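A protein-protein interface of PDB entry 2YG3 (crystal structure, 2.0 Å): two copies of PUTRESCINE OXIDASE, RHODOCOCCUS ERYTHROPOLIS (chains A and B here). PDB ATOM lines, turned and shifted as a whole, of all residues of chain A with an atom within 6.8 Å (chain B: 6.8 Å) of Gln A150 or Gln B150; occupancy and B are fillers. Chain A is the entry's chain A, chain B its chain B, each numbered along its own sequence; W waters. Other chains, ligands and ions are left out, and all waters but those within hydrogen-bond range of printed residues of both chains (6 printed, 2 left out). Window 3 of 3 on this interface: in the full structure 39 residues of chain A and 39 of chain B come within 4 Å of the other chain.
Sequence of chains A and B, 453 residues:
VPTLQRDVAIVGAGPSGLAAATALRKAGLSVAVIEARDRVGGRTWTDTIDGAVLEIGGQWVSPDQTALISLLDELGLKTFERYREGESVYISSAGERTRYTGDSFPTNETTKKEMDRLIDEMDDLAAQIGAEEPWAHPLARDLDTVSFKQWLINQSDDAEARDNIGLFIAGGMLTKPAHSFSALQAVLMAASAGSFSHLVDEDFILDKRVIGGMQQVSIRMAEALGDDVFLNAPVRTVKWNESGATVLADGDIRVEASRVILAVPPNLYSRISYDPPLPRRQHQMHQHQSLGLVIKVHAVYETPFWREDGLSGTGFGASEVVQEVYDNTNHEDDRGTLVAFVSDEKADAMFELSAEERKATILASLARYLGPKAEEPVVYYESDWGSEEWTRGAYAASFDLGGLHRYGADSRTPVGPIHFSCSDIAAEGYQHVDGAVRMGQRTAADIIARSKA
Thr A145 touches Lys B149, and with the chains exchanged Lys A149 touches Thr B145.
Thr A145 touches His B179, and with the chains exchanged His A179 touches Thr B145.
Gln B150 touches its own counterpart, Gln A150.
Of the 5 pairs that touch across the chains among the printed residues, 5 have their exchanged pair printed and touching as well.
The side-chain hydroxyl (OG) of Ser A147 lies within hydrogen-bond range of the backbone NH (N) of Gln A150.
The backbone NH (N) of Lys A149 sits at hydrogen-bond distance from the backbone carbonyl oxygen (O) of Ala A178 (3.0 Å).
The side-chain amide nitrogen (NE2) of Gln A150 is in hydrogen-bond range of the side-chain amide oxygen (OD1) of Asn A154 (2.9 Å).
OG of Ser B147 lies within hydrogen-bond range of N of Gln B150, at 3.1 Å.
O of Ala B178 is in hydrogen-bond range of N of Lys B149 (3.0 Å).
NE2 of Gln B150 sits at hydrogen-bond distance from OD1 of Asn B154 (2.9 Å).
Gln A150 touches one residue of chain B.
Of the printed residues of chain A, Gln B150 touches Gln A150 (3.4 Å).
Of the printed residues of chain B, Thr A145 touches Lys B149 (3.3 Å) and His B179 (3.6 Å).
Printed residues of chain A within 4 Å of His B179: Thr A145 (3.6 Å).
Ser A147 touches none of the printed residues of chain B.
Phe B148 touches none of the printed residues of chain A.
The nearest printed residue of chain A that does not touch His B179 is Val A146 (5.6 Å).
Water W2 lies within hydrogen-bond range of the side-chain hydroxyl of Thr B145 (2.6 Å) and the side-chain amino group of Lys A149 (2.9 Å).
Water W6 lies within hydrogen-bond range of the side-chain amide oxygen of Gln A150 (2.7 Å) and the side-chain amide nitrogen of Asn B154 (3.0 Å).
Water W5 lies within hydrogen-bond range of OE1 of Gln B150 and ND2 of Asn A154.
Water W4 bridges NZ of Lys B149 and O of Thr A145.
Water W1 lies within hydrogen-bond range of the backbone carbonyl oxygen (O) of His B179 (2.8 Å), the backbone carbonyl oxygen (O) of Thr A145 (2.8 Å) and the side-chain hydroxyl (OG) of Ser B147 (3.0 Å).
Water W3 bridges OG1 of Thr A145 (3.1 Å) and NZ of Lys B149 (3.3 Å).
His B179 touches Thr A145.
Lys A149 touches Thr B145.
OE1 of Gln B150 touches CG of Gln A150, at 3.4 Å.
Thr B145 touches His A179.
The side-chain hydroxyl (OG1) of Thr A145 lies within hydrogen-bond range of the side-chain amino group (NZ) of Lys B149.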
ATOM      1  N   THR A 145     -16.610  -4.164  32.874  1.00  0.00           N
ATOM      2  CA  THR A 145     -17.459  -3.077  33.394  1.00  0.00           C
ATOM      3  C   THR A 145     -17.563  -1.908  32.410  1.00  0.00           C
ATOM      4  O   THR A 145     -18.132  -0.858  32.730  1.00  0.00           O
ATOM      5  CB  THR A 145     -16.951  -2.523  34.746  1.00  0.00           C
ATOM      6  OG1 THR A 145     -15.639  -1.992  34.558  1.00  0.00           O
ATOM      7  CG2 THR A 145     -16.944  -3.602  35.835  1.00  0.00           C
ATOM      8  N   VAL A 146     -17.008  -2.087  31.219  1.00  0.00           N
ATOM      9  CA  VAL A 146     -17.120  -1.083  30.164  1.00  0.00           C
ATOM     10  C   VAL A 146     -17.841  -1.760  29.005  1.00  0.00           C
ATOM     11  O   VAL A 146     -17.537  -2.903  28.675  1.00  0.00           O
ATOM     12  CB  VAL A 146     -15.713  -0.526  29.730  1.00  0.00           C
ATOM     13  CG1 VAL A 146     -14.822  -1.627  29.092  1.00  0.00           C
ATOM     14  CG2 VAL A 146     -15.877   0.639  28.777  1.00  0.00           C
ATOM     15  N   SER A 147     -18.794  -1.072  28.376  1.00  0.00           N
ATOM     16  CA  SER A 147     -19.447  -1.663  27.220  1.00  0.00           C
ATOM     17  C   SER A 147     -18.470  -1.724  26.051  1.00  0.00           C
ATOM     18  O   SER A 147     -17.464  -0.996  26.026  1.00  0.00           O
ATOM     19  CB  SER A 147     -20.711  -0.901  26.827  1.00  0.00           C
ATOM     20  OG  SER A 147     -20.377   0.364  26.273  1.00  0.00           O
ATOM     21  N   PHE A 148     -18.727  -2.632  25.114  1.00  0.00           N
ATOM     22  CA  PHE A 148     -17.867  -2.720  23.931  1.00  0.00           C
ATOM     23  C   PHE A 148     -17.947  -1.415  23.123  1.00  0.00           C
ATOM     24  O   PHE A 148     -16.967  -0.991  22.532  1.00  0.00           O
ATOM     25  CB  PHE A 148     -18.218  -3.930  23.065  1.00  0.00           C
ATOM     26  CG  PHE A 148     -17.199  -4.229  21.987  1.00  0.00           C
ATOM     27  CD1 PHE A 148     -15.834  -4.324  22.291  1.00  0.00           C
ATOM     28  CD2 PHE A 148     -17.604  -4.433  20.672  1.00  0.00           C
ATOM     29  CE1 PHE A 148     -14.890  -4.594  21.288  1.00  0.00           C
ATOM     30  CE2 PHE A 148     -16.661  -4.724  19.669  1.00  0.00           C
ATOM     31  CZ  PHE A 148     -15.311  -4.807  19.987  1.00  0.00           C
ATOM     32  N   LYS A 149     -19.117  -0.786  23.117  1.00  0.00           N
ATOM     33  CA  LYS A 149     -19.275   0.485  22.427  1.00  0.00           C
ATOM     34  C   LYS A 149     -18.346   1.553  23.030  1.00  0.00           C
ATOM     35  O   LYS A 149     -17.633   2.252  22.300  1.00  0.00           O
ATOM     36  CB  LYS A 149     -20.721   0.954  22.482  1.00  0.00           C
ATOM     37  CG  LYS A 149     -20.928   2.355  21.875  1.00  0.00           C
ATOM     38  CD  LYS A 149     -22.285   2.941  22.277  1.00  0.00           C
ATOM     39  CE  LYS A 149     -22.584   4.237  21.508  1.00  0.00           C
ATOM     40  NZ  LYS A 149     -23.795   4.917  22.062  1.00  0.00           N
ATOM     41  N   GLN A 150     -18.369   1.666  24.360  1.00  0.00           N
ATOM     42  CA  GLN A 150     -17.549   2.657  25.062  1.00  0.00           C
ATOM     43  C   GLN A 150     -16.061   2.323  24.903  1.00  0.00           C
ATOM     44  O   GLN A 150     -15.243   3.221  24.744  1.00  0.00           O
ATOM     45  CB  GLN A 150     -17.929   2.708  26.542  1.00  0.00           C
ATOM     46  CG  GLN A 150     -17.136   3.740  27.371  1.00  0.00           C
ATOM     47  CD  GLN A 150     -17.386   5.165  26.907  1.00  0.00           C
ATOM     48  OE1 GLN A 150     -18.519   5.612  26.814  1.00  0.00           O
ATOM     49  NE2 GLN A 150     -16.320   5.862  26.576  1.00  0.00           N
ATOM     50  N   TRP A 151     -15.724   1.029  24.934  1.00  0.00           N
ATOM     51  CA  TRP A 151     -14.334   0.584  24.742  1.00  0.00           C
ATOM     52  C   TRP A 151     -13.844   0.988  23.346  1.00  0.00           C
ATOM     53  O   TRP A 151     -12.737   1.497  23.202  1.00  0.00           O
ATOM     54  CB  TRP A 151     -14.206  -0.939  24.932  1.00  0.00           C
ATOM     55  CG  TRP A 151     -12.796  -1.456  24.865  1.00  0.00           C
ATOM     56  CD1 TRP A 151     -11.911  -1.538  25.896  1.00  0.00           C
ATOM     57  CD2 TRP A 151     -12.112  -1.962  23.704  1.00  0.00           C
ATOM     58  NE1 TRP A 151     -10.719  -2.068  25.453  1.00  0.00           N
ATOM     59  CE2 TRP A 151     -10.815  -2.329  24.112  1.00  0.00           C
ATOM     60  CE3 TRP A 151     -12.466  -2.116  22.354  1.00  0.00           C
ATOM     61  CZ2 TRP A 151      -9.865  -2.853  23.226  1.00  0.00           C
ATOM     62  CZ3 TRP A 151     -11.523  -2.647  21.466  1.00  0.00           C
ATOM     63  CH2 TRP A 151     -10.228  -3.000  21.912  1.00  0.00           C
ATOM     64  N   LEU A 152     -14.672   0.762  22.324  1.00  0.00           N
ATOM     65  CA  LEU A 152     -14.345   1.205  20.952  1.00  0.00           C
ATOM     66  C   LEU A 152     -14.143   2.727  20.873  1.00  0.00           C
ATOM     67  O   LEU A 152     -13.200   3.206  20.224  1.00  0.00           O
ATOM     68  CB  LEU A 152     -15.421   0.763  19.956  1.00  0.00           C
ATOM     69  CG  LEU A 152     -15.454  -0.743  19.654  1.00  0.00           C
ATOM     70  CD1 LEU A 152     -16.739  -1.124  18.936  1.00  0.00           C
ATOM     71  CD2 LEU A 152     -14.217  -1.189  18.861  1.00  0.00           C
ATOM     72  N   ILE A 153     -15.005   3.479  21.554  1.00  0.00           N
ATOM     73  CA  ILE A 153     -14.842   4.956  21.638  1.00  0.00           C
ATOM     74  C   ILE A 153     -13.499   5.329  22.299  1.00  0.00           C
ATOM     75  O   ILE A 153     -12.791   6.236  21.818  1.00  0.00           O
ATOM     76  CB  ILE A 153     -16.023   5.640  22.360  1.00  0.00           C
ATOM     77  CG1 ILE A 153     -17.304   5.517  21.514  1.00  0.00           C
ATOM     78  CG2 ILE A 153     -15.705   7.118  22.680  1.00  0.00           C
ATOM     79  CD1 ILE A 153     -18.582   5.771  22.290  1.00  0.00           C
ATOM     80  N   ASN A 154     -13.141   4.606  23.361  1.00  0.00           N
ATOM     81  CA  ASN A 154     -11.881   4.837  24.062  1.00  0.00           C
ATOM     82  C   ASN A 154     -10.675   4.507  23.196  1.00  0.00           C
ATOM     83  O   ASN A 154      -9.616   5.084  23.375  1.00  0.00           O
ATOM     84  CB  ASN A 154     -11.791   4.026  25.373  1.00  0.00           C
ATOM     85  CG  ASN A 154     -12.819   4.455  26.414  1.00  0.00           C
ATOM     86  OD1 ASN A 154     -13.442   5.498  26.292  1.00  0.00           O
ATOM     87  ND2 ASN A 154     -12.996   3.633  27.444  1.00  0.00           N
ATOM     88  N   GLN A 155     -10.826   3.571  22.266  1.00  0.00           N
ATOM     89  CA  GLN A 155      -9.694   3.129  21.445  1.00  0.00           C
ATOM     90  C   GLN A 155      -9.504   3.916  20.157  1.00  0.00           C
ATOM     91  O   GLN A 155      -8.390   4.008  19.647  1.00  0.00           O
ATOM     92  CB  GLN A 155      -9.805   1.644  21.069  1.00  0.00           C
ATOM     93  CG  GLN A 155      -9.860   0.620  22.220  1.00  0.00           C
ATOM     94  CD  GLN A 155      -8.932   0.935  23.371  1.00  0.00           C
ATOM     95  OE1 GLN A 155      -9.386   1.149  24.494  1.00  0.00           O
ATOM     96  NE2 GLN A 155      -7.647   0.971  23.109  1.00  0.00           N
ATOM     97  N   ALA A 178     -23.727  -3.203  20.616  1.00  0.00           N
ATOM     98  CA  ALA A 178     -22.424  -3.026  21.291  1.00  0.00           C
ATOM     99  C   ALA A 178     -22.497  -2.284  22.629  1.00  0.00           C
ATOM    100  O   ALA A 178     -21.616  -2.451  23.479  1.00  0.00           O
ATOM    101  CB  ALA A 178     -21.416  -2.331  20.329  1.00  0.00           C
ATOM    102  N   HIS A 179     -23.536  -1.475  22.831  1.00  0.00           N
ATOM    103  CA  HIS A 179     -23.724  -0.793  24.122  1.00  0.00           C
ATOM    104  C   HIS A 179     -24.235  -1.727  25.233  1.00  0.00           C
ATOM    105  O   HIS A 179     -24.249  -1.349  26.412  1.00  0.00           O
ATOM    106  CB  HIS A 179     -24.659   0.427  23.981  1.00  0.00           C
ATOM    107  CG  HIS A 179     -26.065   0.086  23.572  1.00  0.00           C
ATOM    108  ND1 HIS A 179     -27.029  -0.345  24.466  1.00  0.00           N
ATOM    109  CD2 HIS A 179     -26.678   0.135  22.367  1.00  0.00           C
ATOM    110  CE1 HIS A 179     -28.161  -0.579  23.821  1.00  0.00           C
ATOM    111  NE2 HIS A 179     -27.975  -0.293  22.545  1.00  0.00           N
ATOM    112  N   THR B 145     -27.991   4.193  26.548  1.00  0.00           N
ATOM    113  CA  THR B 145     -26.901   3.425  25.950  1.00  0.00           C
ATOM    114  C   THR B 145     -25.570   3.692  26.656  1.00  0.00           C
ATOM    115  O   THR B 145     -24.519   3.248  26.196  1.00  0.00           O
ATOM    116  CB  THR B 145     -26.750   3.696  24.439  1.00  0.00           C
ATOM    117  OG1 THR B 145     -26.611   5.107  24.223  1.00  0.00           O
ATOM    118  CG2 THR B 145     -27.961   3.161  23.651  1.00  0.00           C
ATOM    119  N   VAL B 146     -25.623   4.441  27.755  1.00  0.00           N
ATOM    120  CA  VAL B 146     -24.449   4.691  28.580  1.00  0.00           C
ATOM    121  C   VAL B 146     -24.731   4.157  29.977  1.00  0.00           C
ATOM    122  O   VAL B 146     -25.829   4.338  30.505  1.00  0.00           O
ATOM    123  CB  VAL B 146     -24.091   6.224  28.613  1.00  0.00           C
ATOM    124  CG1 VAL B 146     -25.168   7.045  29.344  1.00  0.00           C
ATOM    125  CG2 VAL B 146     -22.737   6.455  29.253  1.00  0.00           C
ATOM    126  N   SER B 147     -23.769   3.479  30.601  1.00  0.00           N
ATOM    127  CA  SER B 147     -24.048   2.992  31.957  1.00  0.00           C
ATOM    128  C   SER B 147     -24.103   4.174  32.912  1.00  0.00           C
ATOM    129  O   SER B 147     -23.593   5.243  32.596  1.00  0.00           O
ATOM    130  CB  SER B 147     -23.006   1.972  32.430  1.00  0.00           C
ATOM    131  OG  SER B 147     -21.748   2.596  32.553  1.00  0.00           O
ATOM    132  N   PHE B 148     -24.757   4.000  34.055  1.00  0.00           N
ATOM    133  CA  PHE B 148     -24.807   5.068  35.052  1.00  0.00           C
ATOM    134  C   PHE B 148     -23.391   5.370  35.542  1.00  0.00           C
ATOM    135  O   PHE B 148     -23.051   6.550  35.755  1.00  0.00           O
ATOM    136  CB  PHE B 148     -25.722   4.697  36.221  1.00  0.00           C
ATOM    137  CG  PHE B 148     -26.064   5.863  37.133  1.00  0.00           C
ATOM    138  CD1 PHE B 148     -26.422   7.121  36.599  1.00  0.00           C
ATOM    139  CD2 PHE B 148     -26.044   5.713  38.508  1.00  0.00           C
ATOM    140  CE1 PHE B 148     -26.735   8.207  37.448  1.00  0.00           C
ATOM    141  CE2 PHE B 148     -26.353   6.783  39.360  1.00  0.00           C
ATOM    142  CZ  PHE B 148     -26.710   8.028  38.829  1.00  0.00           C
ATOM    143  N   LYS B 149     -22.570   4.321  35.699  1.00  0.00           N
ATOM    144  CA  LYS B 149     -21.162   4.491  36.079  1.00  0.00           C
ATOM    145  C   LYS B 149     -20.415   5.429  35.108  1.00  0.00           C
ATOM    146  O   LYS B 149     -19.760   6.376  35.554  1.00  0.00           O
ATOM    147  CB  LYS B 149     -20.439   3.141  36.147  1.00  0.00           C
ATOM    148  CG  LYS B 149     -18.936   3.255  36.483  1.00  0.00           C
ATOM    149  CD  LYS B 149     -18.209   1.933  36.283  1.00  0.00           C
ATOM    150  CE  LYS B 149     -16.753   2.008  36.783  1.00  0.00           C
ATOM    151  NZ  LYS B 149     -15.968   0.882  36.206  1.00  0.00           N
ATOM    152  N   GLN B 150     -20.515   5.146  33.809  1.00  0.00           N
ATOM    153  CA  GLN B 150     -19.887   5.944  32.753  1.00  0.00           C
ATOM    154  C   GLN B 150     -20.466   7.352  32.675  1.00  0.00           C
ATOM    155  O   GLN B 150     -19.728   8.310  32.466  1.00  0.00           O
ATOM    156  CB  GLN B 150     -20.002   5.252  31.392  1.00  0.00           C
ATOM    157  CG  GLN B 150     -19.264   5.966  30.243  1.00  0.00           C
ATOM    158  CD  GLN B 150     -17.757   6.023  30.447  1.00  0.00           C
ATOM    159  OE1 GLN B 150     -17.104   4.989  30.580  1.00  0.00           O
ATOM    160  NE2 GLN B 150     -17.194   7.237  30.461  1.00  0.00           N
ATOM    161  N   TRP B 151     -21.784   7.468  32.836  1.00  0.00           N
ATOM    162  CA  TRP B 151     -22.441   8.774  32.863  1.00  0.00           C
ATOM    163  C   TRP B 151     -21.895   9.638  34.018  1.00  0.00           C
ATOM    164  O   TRP B 151     -21.614  10.823  33.822  1.00  0.00           O
ATOM    165  CB  TRP B 151     -23.958   8.616  32.978  1.00  0.00           C
ATOM    166  CG  TRP B 151     -24.718   9.927  32.890  1.00  0.00           C
ATOM    167  CD1 TRP B 151     -25.141  10.556  31.751  1.00  0.00           C
ATOM    168  CD2 TRP B 151     -25.141  10.756  33.987  1.00  0.00           C
ATOM    169  NE1 TRP B 151     -25.804  11.729  32.070  1.00  0.00           N
ATOM    170  CE2 TRP B 151     -25.814  11.874  33.433  1.00  0.00           C
ATOM    171  CE3 TRP B 151     -25.016  10.662  35.376  1.00  0.00           C
ATOM    172  CZ2 TRP B 151     -26.351  12.889  34.224  1.00  0.00           C
ATOM    173  CZ3 TRP B 151     -25.558  11.670  36.165  1.00  0.00           C
ATOM    174  CH2 TRP B 151     -26.217  12.770  35.590  1.00  0.00           C
ATOM    175  N   LEU B 152     -21.737   9.041  35.198  1.00  0.00           N
ATOM    176  CA  LEU B 152     -21.166   9.746  36.354  1.00  0.00           C
ATOM    177  C   LEU B 152     -19.717  10.178  36.090  1.00  0.00           C
ATOM    178  O   LEU B 152     -19.331  11.290  36.464  1.00  0.00           O
ATOM    179  CB  LEU B 152     -21.255   8.909  37.639  1.00  0.00           C
ATOM    180  CG  LEU B 152     -22.658   8.670  38.211  1.00  0.00           C
ATOM    181  CD1 LEU B 152     -22.659   7.555  39.255  1.00  0.00           C
ATOM    182  CD2 LEU B 152     -23.238   9.960  38.773  1.00  0.00           C
ATOM    183  N   ILE B 153     -18.920   9.299  35.472  1.00  0.00           N
ATOM    184  CA  ILE B 153     -17.551   9.644  35.056  1.00  0.00           C
ATOM    185  C   ILE B 153     -17.564  10.826  34.085  1.00  0.00           C
ATOM    186  O   ILE B 153     -16.749  11.741  34.214  1.00  0.00           O
ATOM    187  CB  ILE B 153     -16.791   8.457  34.437  1.00  0.00           C
ATOM    188  CG1 ILE B 153     -16.521   7.378  35.500  1.00  0.00           C
ATOM    189  CG2 ILE B 153     -15.485   8.929  33.761  1.00  0.00           C
ATOM    190  CD1 ILE B 153     -16.060   6.021  34.873  1.00  0.00           C
ATOM    191  N   ASN B 154     -18.506  10.816  33.142  1.00  0.00           N
ATOM    192  CA  ASN B 154     -18.673  11.921  32.208  1.00  0.00           C
ATOM    193  C   ASN B 154     -19.102  13.240  32.858  1.00  0.00           C
ATOM    194  O   ASN B 154     -18.786  14.300  32.328  1.00  0.00           O
ATOM    195  CB  ASN B 154     -19.696  11.574  31.118  1.00  0.00           C
ATOM    196  CG  ASN B 154     -19.236  10.459  30.202  1.00  0.00           C
ATOM    197  OD1 ASN B 154     -18.080  10.029  30.240  1.00  0.00           O
ATOM    198  ND2 ASN B 154     -20.155   9.990  29.336  1.00  0.00           N
ATOM    199  N   GLN B 155     -19.836  13.179  33.964  1.00  0.00           N
ATOM    200  CA  GLN B 155     -20.329  14.383  34.631  1.00  0.00           C
ATOM    201  C   GLN B 155     -19.340  14.977  35.638  1.00  0.00           C
ATOM    202  O   GLN B 155     -19.363  16.187  35.830  1.00  0.00           O
ATOM    203  CB  GLN B 155     -21.657  14.137  35.370  1.00  0.00           C
ATOM    204  CG  GLN B 155     -22.847  13.640  34.520  1.00  0.00           C
ATOM    205  CD  GLN B 155     -22.913  14.263  33.150  1.00  0.00           C
ATOM    206  OE1 GLN B 155     -22.757  13.574  32.141  1.00  0.00           O
ATOM    207  NE2 GLN B 155     -23.133  15.563  33.095  1.00  0.00           N
ATOM    208  N   ALA B 178     -23.496  -0.084  39.302  1.00  0.00           N
ATOM    209  CA  ALA B 178     -23.746   1.063  38.417  1.00  0.00           C
ATOM    210  C   ALA B 178     -23.240   0.872  36.984  1.00  0.00           C
ATOM    211  O   ALA B 178     -23.700   1.552  36.067  1.00  0.00           O
ATOM    212  CB  ALA B 178     -23.150   2.356  39.033  1.00  0.00           C
ATOM    213  N   HIS B 179     -22.298  -0.044  36.795  1.00  0.00           N
ATOM    214  CA  HIS B 179     -21.845  -0.383  35.440  1.00  0.00           C
ATOM    215  C   HIS B 179     -22.857  -1.239  34.665  1.00  0.00           C
ATOM    216  O   HIS B 179     -22.692  -1.444  33.465  1.00  0.00           O
ATOM    217  CB  HIS B 179     -20.454  -1.058  35.477  1.00  0.00           C
ATOM    218  CG  HIS B 179     -20.417  -2.363  36.220  1.00  0.00           C
ATOM    219  ND1 HIS B 179     -20.764  -3.565  35.631  1.00  0.00           N
ATOM    220  CD2 HIS B 179     -20.039  -2.663  37.483  1.00  0.00           C
ATOM    221  CE1 HIS B 179     -20.627  -4.542  36.510  1.00  0.00           C
ATOM    222  NE2 HIS B 179     -20.179  -4.021  37.636  1.00  0.00           N
HETATM  223  O   HOH W   1     -20.743  -0.139  31.985  1.00  0.00           O
HETATM  224  O   HOH W   2     -26.400   6.207  21.919  1.00  0.00           O
HETATM  225  O   HOH W   3     -13.807  -1.552  36.973  1.00  0.00           O
HETATM  226  O   HOH W   4     -15.887   1.095  33.451  1.00  0.00           O
HETATM  227  O   HOH W   5     -14.552   4.480  29.807  1.00  0.00           O
HETATM  228  O   HOH W   6     -19.472   8.130  27.142  1.00  0.00           O
